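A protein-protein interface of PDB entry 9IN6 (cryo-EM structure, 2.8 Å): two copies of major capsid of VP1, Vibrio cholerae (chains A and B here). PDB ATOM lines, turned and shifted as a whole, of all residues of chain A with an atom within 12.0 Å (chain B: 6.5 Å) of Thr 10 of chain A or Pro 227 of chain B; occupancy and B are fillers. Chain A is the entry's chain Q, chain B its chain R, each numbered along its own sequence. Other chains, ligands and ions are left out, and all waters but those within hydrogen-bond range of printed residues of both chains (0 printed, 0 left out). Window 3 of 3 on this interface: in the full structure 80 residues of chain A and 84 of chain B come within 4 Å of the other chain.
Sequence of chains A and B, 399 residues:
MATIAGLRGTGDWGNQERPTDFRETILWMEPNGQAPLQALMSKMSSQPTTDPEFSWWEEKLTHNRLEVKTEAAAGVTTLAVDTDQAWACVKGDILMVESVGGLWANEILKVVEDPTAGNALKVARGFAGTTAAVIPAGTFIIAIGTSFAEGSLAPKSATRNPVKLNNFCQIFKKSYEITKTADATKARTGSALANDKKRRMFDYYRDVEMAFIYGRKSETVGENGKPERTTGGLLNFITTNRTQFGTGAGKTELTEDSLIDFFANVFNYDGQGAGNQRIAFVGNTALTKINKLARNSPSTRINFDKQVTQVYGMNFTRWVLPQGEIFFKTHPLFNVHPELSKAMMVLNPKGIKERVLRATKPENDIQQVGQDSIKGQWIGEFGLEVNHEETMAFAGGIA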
ATOM      1  N   ILE A   4      24.246 -23.793 -29.695  1.00  0.00           N
ATOM      2  CA  ILE A   4      23.835 -24.097 -28.332  1.00  0.00           C
ATOM      3  C   ILE A   4      24.447 -25.438 -27.965  1.00  0.00           C
ATOM      4  O   ILE A   4      24.487 -26.351 -28.797  1.00  0.00           O
ATOM      5  CB  ILE A   4      22.300 -24.122 -28.200  1.00  0.00           C
ATOM      6  CG1 ILE A   4      21.733 -22.715 -28.395  1.00  0.00           C
ATOM      7  CG2 ILE A   4      21.883 -24.678 -26.854  1.00  0.00           C
ATOM      8  CD1 ILE A   4      20.410 -22.680 -29.118  1.00  0.00           C
ATOM      9  N   ALA A   5      24.938 -25.554 -26.738  1.00  0.00           N
ATOM     10  CA  ALA A   5      25.628 -26.753 -26.289  1.00  0.00           C
ATOM     11  C   ALA A   5      24.659 -27.925 -26.266  1.00  0.00           C
ATOM     12  O   ALA A   5      23.746 -27.967 -25.436  1.00  0.00           O
ATOM     13  CB  ALA A   5      26.237 -26.540 -24.903  1.00  0.00           C
ATOM     14  N   GLY A   6      24.863 -28.875 -27.169  1.00  0.00           N
ATOM     15  CA  GLY A   6      24.015 -30.045 -27.230  1.00  0.00           C
ATOM     16  C   GLY A   6      22.878 -29.914 -28.221  1.00  0.00           C
ATOM     17  O   GLY A   6      22.792 -28.979 -29.020  1.00  0.00           O
ATOM     18  N   LEU A   7      21.985 -30.896 -28.159  1.00  0.00           N
ATOM     19  CA  LEU A   7      20.861 -30.951 -29.080  1.00  0.00           C
ATOM     20  C   LEU A   7      19.828 -29.879 -28.746  1.00  0.00           C
ATOM     21  O   LEU A   7      19.776 -29.360 -27.629  1.00  0.00           O
ATOM     22  CB  LEU A   7      20.221 -32.339 -29.050  1.00  0.00           C
ATOM     23  CG  LEU A   7      19.269 -32.719 -27.915  1.00  0.00           C
ATOM     24  CD1 LEU A   7      18.496 -33.959 -28.303  1.00  0.00           C
ATOM     25  CD2 LEU A   7      20.007 -32.948 -26.611  1.00  0.00           C
ATOM     26  N   ARG A   8      19.008 -29.542 -29.736  1.00  0.00           N
ATOM     27  CA  ARG A   8      18.028 -28.476 -29.586  1.00  0.00           C
ATOM     28  C   ARG A   8      16.769 -28.980 -28.893  1.00  0.00           C
ATOM     29  O   ARG A   8      16.280 -30.075 -29.178  1.00  0.00           O
ATOM     30  CB  ARG A   8      17.666 -27.887 -30.948  1.00  0.00           C
ATOM     31  CG  ARG A   8      16.736 -26.690 -30.873  1.00  0.00           C
ATOM     32  CD  ARG A   8      16.358 -26.186 -32.249  1.00  0.00           C
ATOM     33  NE  ARG A   8      17.417 -25.376 -32.834  1.00  0.00           N
ATOM     34  CZ  ARG A   8      17.542 -24.069 -32.662  1.00  0.00           C
ATOM     35  NH1 ARG A   8      16.684 -23.386 -31.925  1.00  0.00           N
ATOM     36  NH2 ARG A   8      18.554 -23.432 -33.240  1.00  0.00           N
ATOM     37  N   GLY A   9      16.244 -28.164 -27.978  1.00  0.00           N
ATOM     38  CA  GLY A   9      15.005 -28.463 -27.292  1.00  0.00           C
ATOM     39  C   GLY A   9      14.041 -27.292 -27.372  1.00  0.00           C
ATOM     40  O   GLY A   9      14.334 -26.267 -27.988  1.00  0.00           O
ATOM     41  N   THR A  10      12.885 -27.471 -26.731  1.00  0.00           N
ATOM     42  CA  THR A  10      11.864 -26.430 -26.755  1.00  0.00           C
ATOM     43  C   THR A  10      12.267 -25.199 -25.957  1.00  0.00           C
ATOM     44  O   THR A  10      11.648 -24.145 -26.118  1.00  0.00           O
ATOM     45  CB  THR A  10      10.534 -26.965 -26.230  1.00  0.00           C
ATOM     46  OG1 THR A  10      10.683 -27.365 -24.864  1.00  0.00           O
ATOM     47  CG2 THR A  10      10.082 -28.144 -27.054  1.00  0.00           C
ATOM     48  N   GLY A  11      13.272 -25.307 -25.102  1.00  0.00           N
ATOM     49  CA  GLY A  11      13.771 -24.170 -24.365  1.00  0.00           C
ATOM     50  C   GLY A  11      14.958 -23.480 -24.992  1.00  0.00           C
ATOM     51  O   GLY A  11      15.679 -22.760 -24.294  1.00  0.00           O
ATOM     52  N   ASP A  12      15.192 -23.677 -26.288  1.00  0.00           N
ATOM     53  CA  ASP A  12      16.399 -23.198 -26.941  1.00  0.00           C
ATOM     54  C   ASP A  12      16.155 -22.114 -27.980  1.00  0.00           C
ATOM     55  O   ASP A  12      17.123 -21.556 -28.499  1.00  0.00           O
ATOM     56  CB  ASP A  12      17.138 -24.366 -27.594  1.00  0.00           C
ATOM     57  CG  ASP A  12      17.811 -25.262 -26.581  1.00  0.00           C
ATOM     58  OD1 ASP A  12      18.364 -24.729 -25.598  1.00  0.00           O
ATOM     59  OD2 ASP A  12      17.785 -26.495 -26.764  1.00  0.00           O
ATOM     60  N   TRP A  13      14.905 -21.800 -28.308  1.00  0.00           N
ATOM     61  CA  TRP A  13      14.691 -20.670 -29.197  1.00  0.00           C
ATOM     62  C   TRP A  13      15.005 -19.360 -28.488  1.00  0.00           C
ATOM     63  O   TRP A  13      15.063 -19.280 -27.259  1.00  0.00           O
ATOM     64  CB  TRP A  13      13.257 -20.621 -29.723  1.00  0.00           C
ATOM     65  CG  TRP A  13      12.932 -21.631 -30.768  1.00  0.00           C
ATOM     66  CD1 TRP A  13      13.183 -21.528 -32.099  1.00  0.00           C
ATOM     67  CD2 TRP A  13      12.210 -22.853 -30.592  1.00  0.00           C
ATOM     68  NE1 TRP A  13      12.709 -22.630 -32.760  1.00  0.00           N
ATOM     69  CE2 TRP A  13      12.103 -23.459 -31.856  1.00  0.00           C
ATOM     70  CE3 TRP A  13      11.665 -23.504 -29.486  1.00  0.00           C
ATOM     71  CZ2 TRP A  13      11.471 -24.680 -32.044  1.00  0.00           C
ATOM     72  CZ3 TRP A  13      11.037 -24.714 -29.676  1.00  0.00           C
ATOM     73  CH2 TRP A  13      10.946 -25.292 -30.944  1.00  0.00           C
ATOM     74  N   GLY A  14      15.210 -18.321 -29.287  1.00  0.00           N
ATOM     75  CA  GLY A  14      15.428 -16.993 -28.765  1.00  0.00           C
ATOM     76  C   GLY A  14      14.126 -16.340 -28.351  1.00  0.00           C
ATOM     77  O   GLY A  14      13.055 -16.949 -28.345  1.00  0.00           O
ATOM     78  N   ASN A  15      14.231 -15.065 -28.000  1.00  0.00           N
ATOM     79  CA  ASN A  15      13.073 -14.331 -27.515  1.00  0.00           C
ATOM     80  C   ASN A  15      12.005 -14.243 -28.598  1.00  0.00           C
ATOM     81  O   ASN A  15      12.294 -13.904 -29.747  1.00  0.00           O
ATOM     82  CB  ASN A  15      13.497 -12.933 -27.071  1.00  0.00           C
ATOM     83  CG  ASN A  15      12.353 -12.140 -26.488  1.00  0.00           C
ATOM     84  OD1 ASN A  15      11.342 -12.701 -26.073  1.00  0.00           O
ATOM     85  ND2 ASN A  15      12.501 -10.823 -26.459  1.00  0.00           N
ATOM     86  N   GLN A  16      10.768 -14.575 -28.222  1.00  0.00           N
ATOM     87  CA  GLN A  16       9.584 -14.435 -29.065  1.00  0.00           C
ATOM     88  C   GLN A  16       9.585 -15.338 -30.291  1.00  0.00           C
ATOM     89  O   GLN A  16       8.641 -15.298 -31.084  1.00  0.00           O
ATOM     90  CB  GLN A  16       9.411 -12.981 -29.515  1.00  0.00           C
ATOM     91  CG  GLN A  16       9.295 -11.988 -28.384  1.00  0.00           C
ATOM     92  CD  GLN A  16       7.878 -11.854 -27.869  1.00  0.00           C
ATOM     93  OE1 GLN A  16       7.027 -12.702 -28.129  1.00  0.00           O
ATOM     94  NE2 GLN A  16       7.618 -10.780 -27.136  1.00  0.00           N
ATOM     95  N   GLU A  17      10.625 -16.152 -30.471  1.00  0.00           N
ATOM     96  CA  GLU A  17      10.630 -17.078 -31.599  1.00  0.00           C
ATOM     97  C   GLU A  17       9.551 -18.137 -31.448  1.00  0.00           C
ATOM     98  O   GLU A  17       8.863 -18.474 -32.416  1.00  0.00           O
ATOM     99  CB  GLU A  17      11.998 -17.740 -31.739  1.00  0.00           C
ATOM    100  CG  GLU A  17      13.081 -16.829 -32.252  1.00  0.00           C
ATOM    101  CD  GLU A  17      14.269 -17.600 -32.774  1.00  0.00           C
ATOM    102  OE1 GLU A  17      14.073 -18.473 -33.643  1.00  0.00           O
ATOM    103  OE2 GLU A  17      15.396 -17.340 -32.306  1.00  0.00           O
ATOM    104  N   ARG A  18       9.388 -18.667 -30.244  1.00  0.00           N
ATOM    105  CA  ARG A  18       8.413 -19.717 -29.985  1.00  0.00           C
ATOM    106  C   ARG A  18       7.238 -19.146 -29.209  1.00  0.00           C
ATOM    107  O   ARG A  18       7.403 -18.763 -28.040  1.00  0.00           O
ATOM    108  CB  ARG A  18       9.061 -20.861 -29.207  1.00  0.00           C
ATOM    109  CG  ARG A  18       8.088 -21.759 -28.470  1.00  0.00           C
ATOM    110  CD  ARG A  18       8.785 -22.464 -27.326  1.00  0.00           C
ATOM    111  NE  ARG A  18       7.837 -23.094 -26.416  1.00  0.00           N
ATOM    112  CZ  ARG A  18       8.156 -23.588 -25.230  1.00  0.00           C
ATOM    113  NH1 ARG A  18       9.395 -23.531 -24.769  1.00  0.00           N
ATOM    114  NH2 ARG A  18       7.211 -24.152 -24.487  1.00  0.00           N
ATOM    115  N   PRO A  19       6.058 -19.034 -29.807  1.00  0.00           N
ATOM    116  CA  PRO A  19       4.854 -18.758 -29.027  1.00  0.00           C
ATOM    117  C   PRO A  19       4.198 -20.053 -28.586  1.00  0.00           C
ATOM    118  O   PRO A  19       4.358 -21.108 -29.201  1.00  0.00           O
ATOM    119  CB  PRO A  19       3.972 -18.000 -30.026  1.00  0.00           C
ATOM    120  CG  PRO A  19       4.338 -18.599 -31.339  1.00  0.00           C
ATOM    121  CD  PRO A  19       5.780 -19.048 -31.252  1.00  0.00           C
ATOM    122  N   THR A  20       3.454 -19.964 -27.496  1.00  0.00           N
ATOM    123  CA  THR A  20       2.760 -21.128 -26.975  1.00  0.00           C
ATOM    124  C   THR A  20       1.401 -21.250 -27.663  1.00  0.00           C
ATOM    125  O   THR A  20       1.112 -20.551 -28.637  1.00  0.00           O
ATOM    126  CB  THR A  20       2.653 -21.032 -25.459  1.00  0.00           C
ATOM    127  OG1 THR A  20       1.894 -19.870 -25.109  1.00  0.00           O
ATOM    128  CG2 THR A  20       4.037 -20.919 -24.852  1.00  0.00           C
ATOM    129  N   ASP A  21       0.556 -22.151 -27.175  1.00  0.00           N
ATOM    130  CA  ASP A  21      -0.753 -22.395 -27.766  1.00  0.00           C
ATOM    131  C   ASP A  21      -1.818 -21.666 -26.963  1.00  0.00           C
ATOM    132  O   ASP A  21      -1.806 -21.707 -25.730  1.00  0.00           O
ATOM    133  CB  ASP A  21      -1.056 -23.891 -27.813  1.00  0.00           C
ATOM    134  CG  ASP A  21      -2.263 -24.212 -28.663  1.00  0.00           C
ATOM    135  OD1 ASP A  21      -2.126 -24.271 -29.900  1.00  0.00           O
ATOM    136  OD2 ASP A  21      -3.354 -24.405 -28.094  1.00  0.00           O
ATOM    137  N   ASP B  51       1.947 -26.837 -28.967  1.00  0.00           N
ATOM    138  CA  ASP B  51       3.026 -26.556 -28.038  1.00  0.00           C
ATOM    139  C   ASP B  51       2.867 -27.445 -26.815  1.00  0.00           C
ATOM    140  O   ASP B  51       1.750 -27.863 -26.494  1.00  0.00           O
ATOM    141  CB  ASP B  51       3.025 -25.081 -27.609  1.00  0.00           C
ATOM    142  CG  ASP B  51       4.362 -24.625 -27.068  1.00  0.00           C
ATOM    143  OD1 ASP B  51       5.343 -24.630 -27.834  1.00  0.00           O
ATOM    144  OD2 ASP B  51       4.437 -24.266 -25.878  1.00  0.00           O
ATOM    145  N   PRO B  52       3.965 -27.760 -26.123  1.00  0.00           N
ATOM    146  CA  PRO B  52       3.839 -28.453 -24.834  1.00  0.00           C
ATOM    147  C   PRO B  52       3.126 -27.635 -23.773  1.00  0.00           C
ATOM    148  O   PRO B  52       2.855 -28.167 -22.692  1.00  0.00           O
ATOM    149  CB  PRO B  52       5.294 -28.726 -24.436  1.00  0.00           C
ATOM    150  CG  PRO B  52       6.038 -28.715 -25.711  1.00  0.00           C
ATOM    151  CD  PRO B  52       5.356 -27.731 -26.598  1.00  0.00           C
ATOM    152  N   GLU B 219       7.530 -27.951 -13.838  1.00  0.00           N
ATOM    153  CA  GLU B 219       8.514 -27.974 -14.911  1.00  0.00           C
ATOM    154  C   GLU B 219       9.905 -27.824 -14.319  1.00  0.00           C
ATOM    155  O   GLU B 219      10.152 -26.899 -13.540  1.00  0.00           O
ATOM    156  CB  GLU B 219       8.263 -26.863 -15.930  1.00  0.00           C
ATOM    157  CG  GLU B 219       9.188 -26.931 -17.127  1.00  0.00           C
ATOM    158  CD  GLU B 219       8.734 -26.046 -18.266  1.00  0.00           C
ATOM    159  OE1 GLU B 219       7.717 -25.344 -18.105  1.00  0.00           O
ATOM    160  OE2 GLU B 219       9.391 -26.055 -19.325  1.00  0.00           O
ATOM    161  N   THR B 220      10.809 -28.726 -14.692  1.00  0.00           N
ATOM    162  CA  THR B 220      12.169 -28.723 -14.178  1.00  0.00           C
ATOM    163  C   THR B 220      13.131 -29.078 -15.302  1.00  0.00           C
ATOM    164  O   THR B 220      12.731 -29.322 -16.441  1.00  0.00           O
ATOM    165  CB  THR B 220      12.343 -29.709 -13.018  1.00  0.00           C
ATOM    166  OG1 THR B 220      11.799 -30.981 -13.386  1.00  0.00           O
ATOM    167  CG2 THR B 220      11.643 -29.202 -11.771  1.00  0.00           C
ATOM    168  N   VAL B 221      14.413 -29.110 -14.962  1.00  0.00           N
ATOM    169  CA  VAL B 221      15.460 -29.480 -15.903  1.00  0.00           C
ATOM    170  C   VAL B 221      15.860 -30.926 -15.643  1.00  0.00           C
ATOM    171  O   VAL B 221      16.178 -31.298 -14.507  1.00  0.00           O
ATOM    172  CB  VAL B 221      16.666 -28.536 -15.780  1.00  0.00           C
ATOM    173  CG1 VAL B 221      17.909 -29.182 -16.352  1.00  0.00           C
ATOM    174  CG2 VAL B 221      16.375 -27.229 -16.488  1.00  0.00           C
ATOM    175  N   GLY B 222      15.841 -31.742 -16.692  1.00  0.00           N
ATOM    176  CA  GLY B 222      16.142 -33.148 -16.562  1.00  0.00           C
ATOM    177  C   GLY B 222      17.624 -33.420 -16.413  1.00  0.00           C
ATOM    178  O   GLY B 222      18.463 -32.521 -16.399  1.00  0.00           O
ATOM    179  N   ASN B 224      19.617 -34.651 -18.484  1.00  0.00           N
ATOM    180  CA  ASN B 224      20.373 -34.295 -19.673  1.00  0.00           C
ATOM    181  C   ASN B 224      20.283 -32.810 -20.003  1.00  0.00           C
ATOM    182  O   ASN B 224      20.654 -32.408 -21.108  1.00  0.00           O
ATOM    183  CB  ASN B 224      19.908 -35.124 -20.870  1.00  0.00           C
ATOM    184  CG  ASN B 224      18.478 -34.835 -21.260  1.00  0.00           C
ATOM    185  OD1 ASN B 224      17.722 -34.242 -20.493  1.00  0.00           O
ATOM    186  ND2 ASN B 224      18.097 -35.250 -22.460  1.00  0.00           N
ATOM    187  N   GLY B 225      19.790 -31.992 -19.077  1.00  0.00           N
ATOM    188  CA  GLY B 225      19.696 -30.566 -19.304  1.00  0.00           C
ATOM    189  C   GLY B 225      18.482 -30.112 -20.078  1.00  0.00           C
ATOM    190  O   GLY B 225      18.397 -28.930 -20.424  1.00  0.00           O
ATOM    191  N   LYS B 226      17.544 -31.003 -20.360  1.00  0.00           N
ATOM    192  CA  LYS B 226      16.356 -30.689 -21.129  1.00  0.00           C
ATOM    193  C   LYS B 226      15.130 -30.613 -20.223  1.00  0.00           C
ATOM    194  O   LYS B 226      15.106 -31.231 -19.155  1.00  0.00           O
ATOM    195  CB  LYS B 226      16.130 -31.743 -22.218  1.00  0.00           C
ATOM    196  CG  LYS B 226      17.172 -31.712 -23.317  1.00  0.00           C
ATOM    197  CD  LYS B 226      16.934 -30.545 -24.244  1.00  0.00           C
ATOM    198  CE  LYS B 226      18.225 -30.058 -24.864  1.00  0.00           C
ATOM    199  NZ  LYS B 226      19.241 -29.714 -23.842  1.00  0.00           N
ATOM    200  N   PRO B 227      14.107 -29.848 -20.605  1.00  0.00           N
ATOM    201  CA  PRO B 227      12.959 -29.656 -19.712  1.00  0.00           C
ATOM    202  C   PRO B 227      12.206 -30.949 -19.443  1.00  0.00           C
ATOM    203  O   PRO B 227      12.042 -31.793 -20.326  1.00  0.00           O
ATOM    204  CB  PRO B 227      12.086 -28.648 -20.470  1.00  0.00           C
ATOM    205  CG  PRO B 227      12.524 -28.742 -21.880  1.00  0.00           C
ATOM    206  CD  PRO B 227      13.974 -29.073 -21.848  1.00  0.00           C
ATOM    207  N   GLU B 228      11.735 -31.086 -18.208  1.00  0.00           N
ATOM    208  CA  GLU B 228      10.876 -32.185 -17.789  1.00  0.00           C
ATOM    209  C   GLU B 228       9.579 -31.604 -17.248  1.00  0.00           C
ATOM    210  O   GLU B 228       9.606 -30.722 -16.386  1.00  0.00           O
ATOM    211  CB  GLU B 228      11.559 -33.040 -16.725  1.00  0.00           C
ATOM    212  CG  GLU B 228      10.742 -34.227 -16.282  1.00  0.00           C
ATOM    213  CD  GLU B 228      11.562 -35.230 -15.510  1.00  0.00           C
ATOM    214  OE1 GLU B 228      12.719 -34.913 -15.173  1.00  0.00           O
ATOM    215  OE2 GLU B 228      11.052 -36.337 -15.242  1.00  0.00           O
ATOM    216  N   ARG B 229       8.450 -32.100 -17.745  1.00  0.00           N
ATOM    217  CA  ARG B 229       7.156 -31.499 -17.459  1.00  0.00           C
ATOM    218  C   ARG B 229       6.170 -32.553 -16.984  1.00  0.00           C
ATOM    219  O   ARG B 229       6.214 -33.702 -17.431  1.00  0.00           O
ATOM    220  CB  ARG B 229       6.603 -30.791 -18.695  1.00  0.00           C
ATOM    221  CG  ARG B 229       7.165 -29.403 -18.905  1.00  0.00           C
ATOM    222  CD  ARG B 229       6.588 -28.752 -20.145  1.00  0.00           C
ATOM    223  NE  ARG B 229       7.254 -29.210 -21.359  1.00  0.00           N
ATOM    224  CZ  ARG B 229       8.172 -28.516 -22.015  1.00  0.00           C
ATOM    225  NH1 ARG B 229       8.554 -27.318 -21.607  1.00  0.00           N
ATOM    226  NH2 ARG B 229       8.720 -29.038 -23.107  1.00  0.00           N
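The side-chain hydroxyl of Thr 10 of chain A lies within hydrogen-bond range of the guanidinium group of Arg 229 of chain B (3.1 Å).
NH2 of Arg 18 of chain A is in salt-bridge range of OD2 of Asp 51 of chain B (3.1 Å).
O of Thr 10 of chain A lies within hydrogen-bond range of NH1 of Arg 18 of chain A (2.7 Å).
The side-chain amide oxygen of Asn 224 of chain B is in hydrogen-bond range of the backbone NH of Lys 226 of chain B (3.2 Å).
The guanidinium group (NH1) of Arg 229 of chain B lies within salt-bridge range of the side-chain carboxylate (OE2) of Glu 219 of chain B (2.7 Å).
Leu 7 of chain A touches Lys 226 of chain B.
Thr 10 of chain A touches Pro 227 of chain B (OG1 to CG, 3.8 Å).
Pro 19 of chain A touches Asp 51 of chain B.
Asp 51 of chain B touches Thr 20 of chain A.
Asp 21 of chain A touches Asp 51 of chain B.
Thr 10 of chain A touches two residues of chain B.
Pro 227 of chain B touches one residue of chain A.
No residue of chain A comes within 4 Å of Thr 220 of chain B.
No residue of chain A comes within 4 Å of Val 221 of chain B.
No residue of chain A comes within 4 Å of Gly 222 of chain B.
No residue of chain A comes within 4 Å of Asn 224 of chain B.
No residue of chain A comes within 4 Å of Gly 225 of chain B.
Lys 226 of chain B touches just one residue of chain A: Leu 7 (3.2 Å).
Glu 228 of chain B touches none of the printed residues of chain A.
Arg 229 of chain B touches one residue of chain A.
Of the printed residues of chain B, Asp 21 of chain A touches Asp 51 (3.9 Å).
Of the printed residues of chain B, Thr 20 of chain A touches Asp 51 (3.5 Å).
Of the printed residues of chain B, Leu 7 of chain A touches Lys 226 (3.2 Å).
Pro 52 of chain B touches none of the printed residues of chain A.
Of the 12 printed residues of chain B, 4 touch a printed residue of chain A.
Printed residues of chain A that touch a printed residue of chain B: Leu 7, Thr 10, Arg 18, Pro 19, Thr 20 and Asp 21.
Hydrophobic or aromatic side chains of chain A within 4 Å of the printed part of chain B: Leu 7.
Among the printed residues, 7 pairs touch across the chains.
No position is printed for both chains.
Of the 7 pairs that touch across the chains among the printed residues, none has its exchanged pair printed and touching as well.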
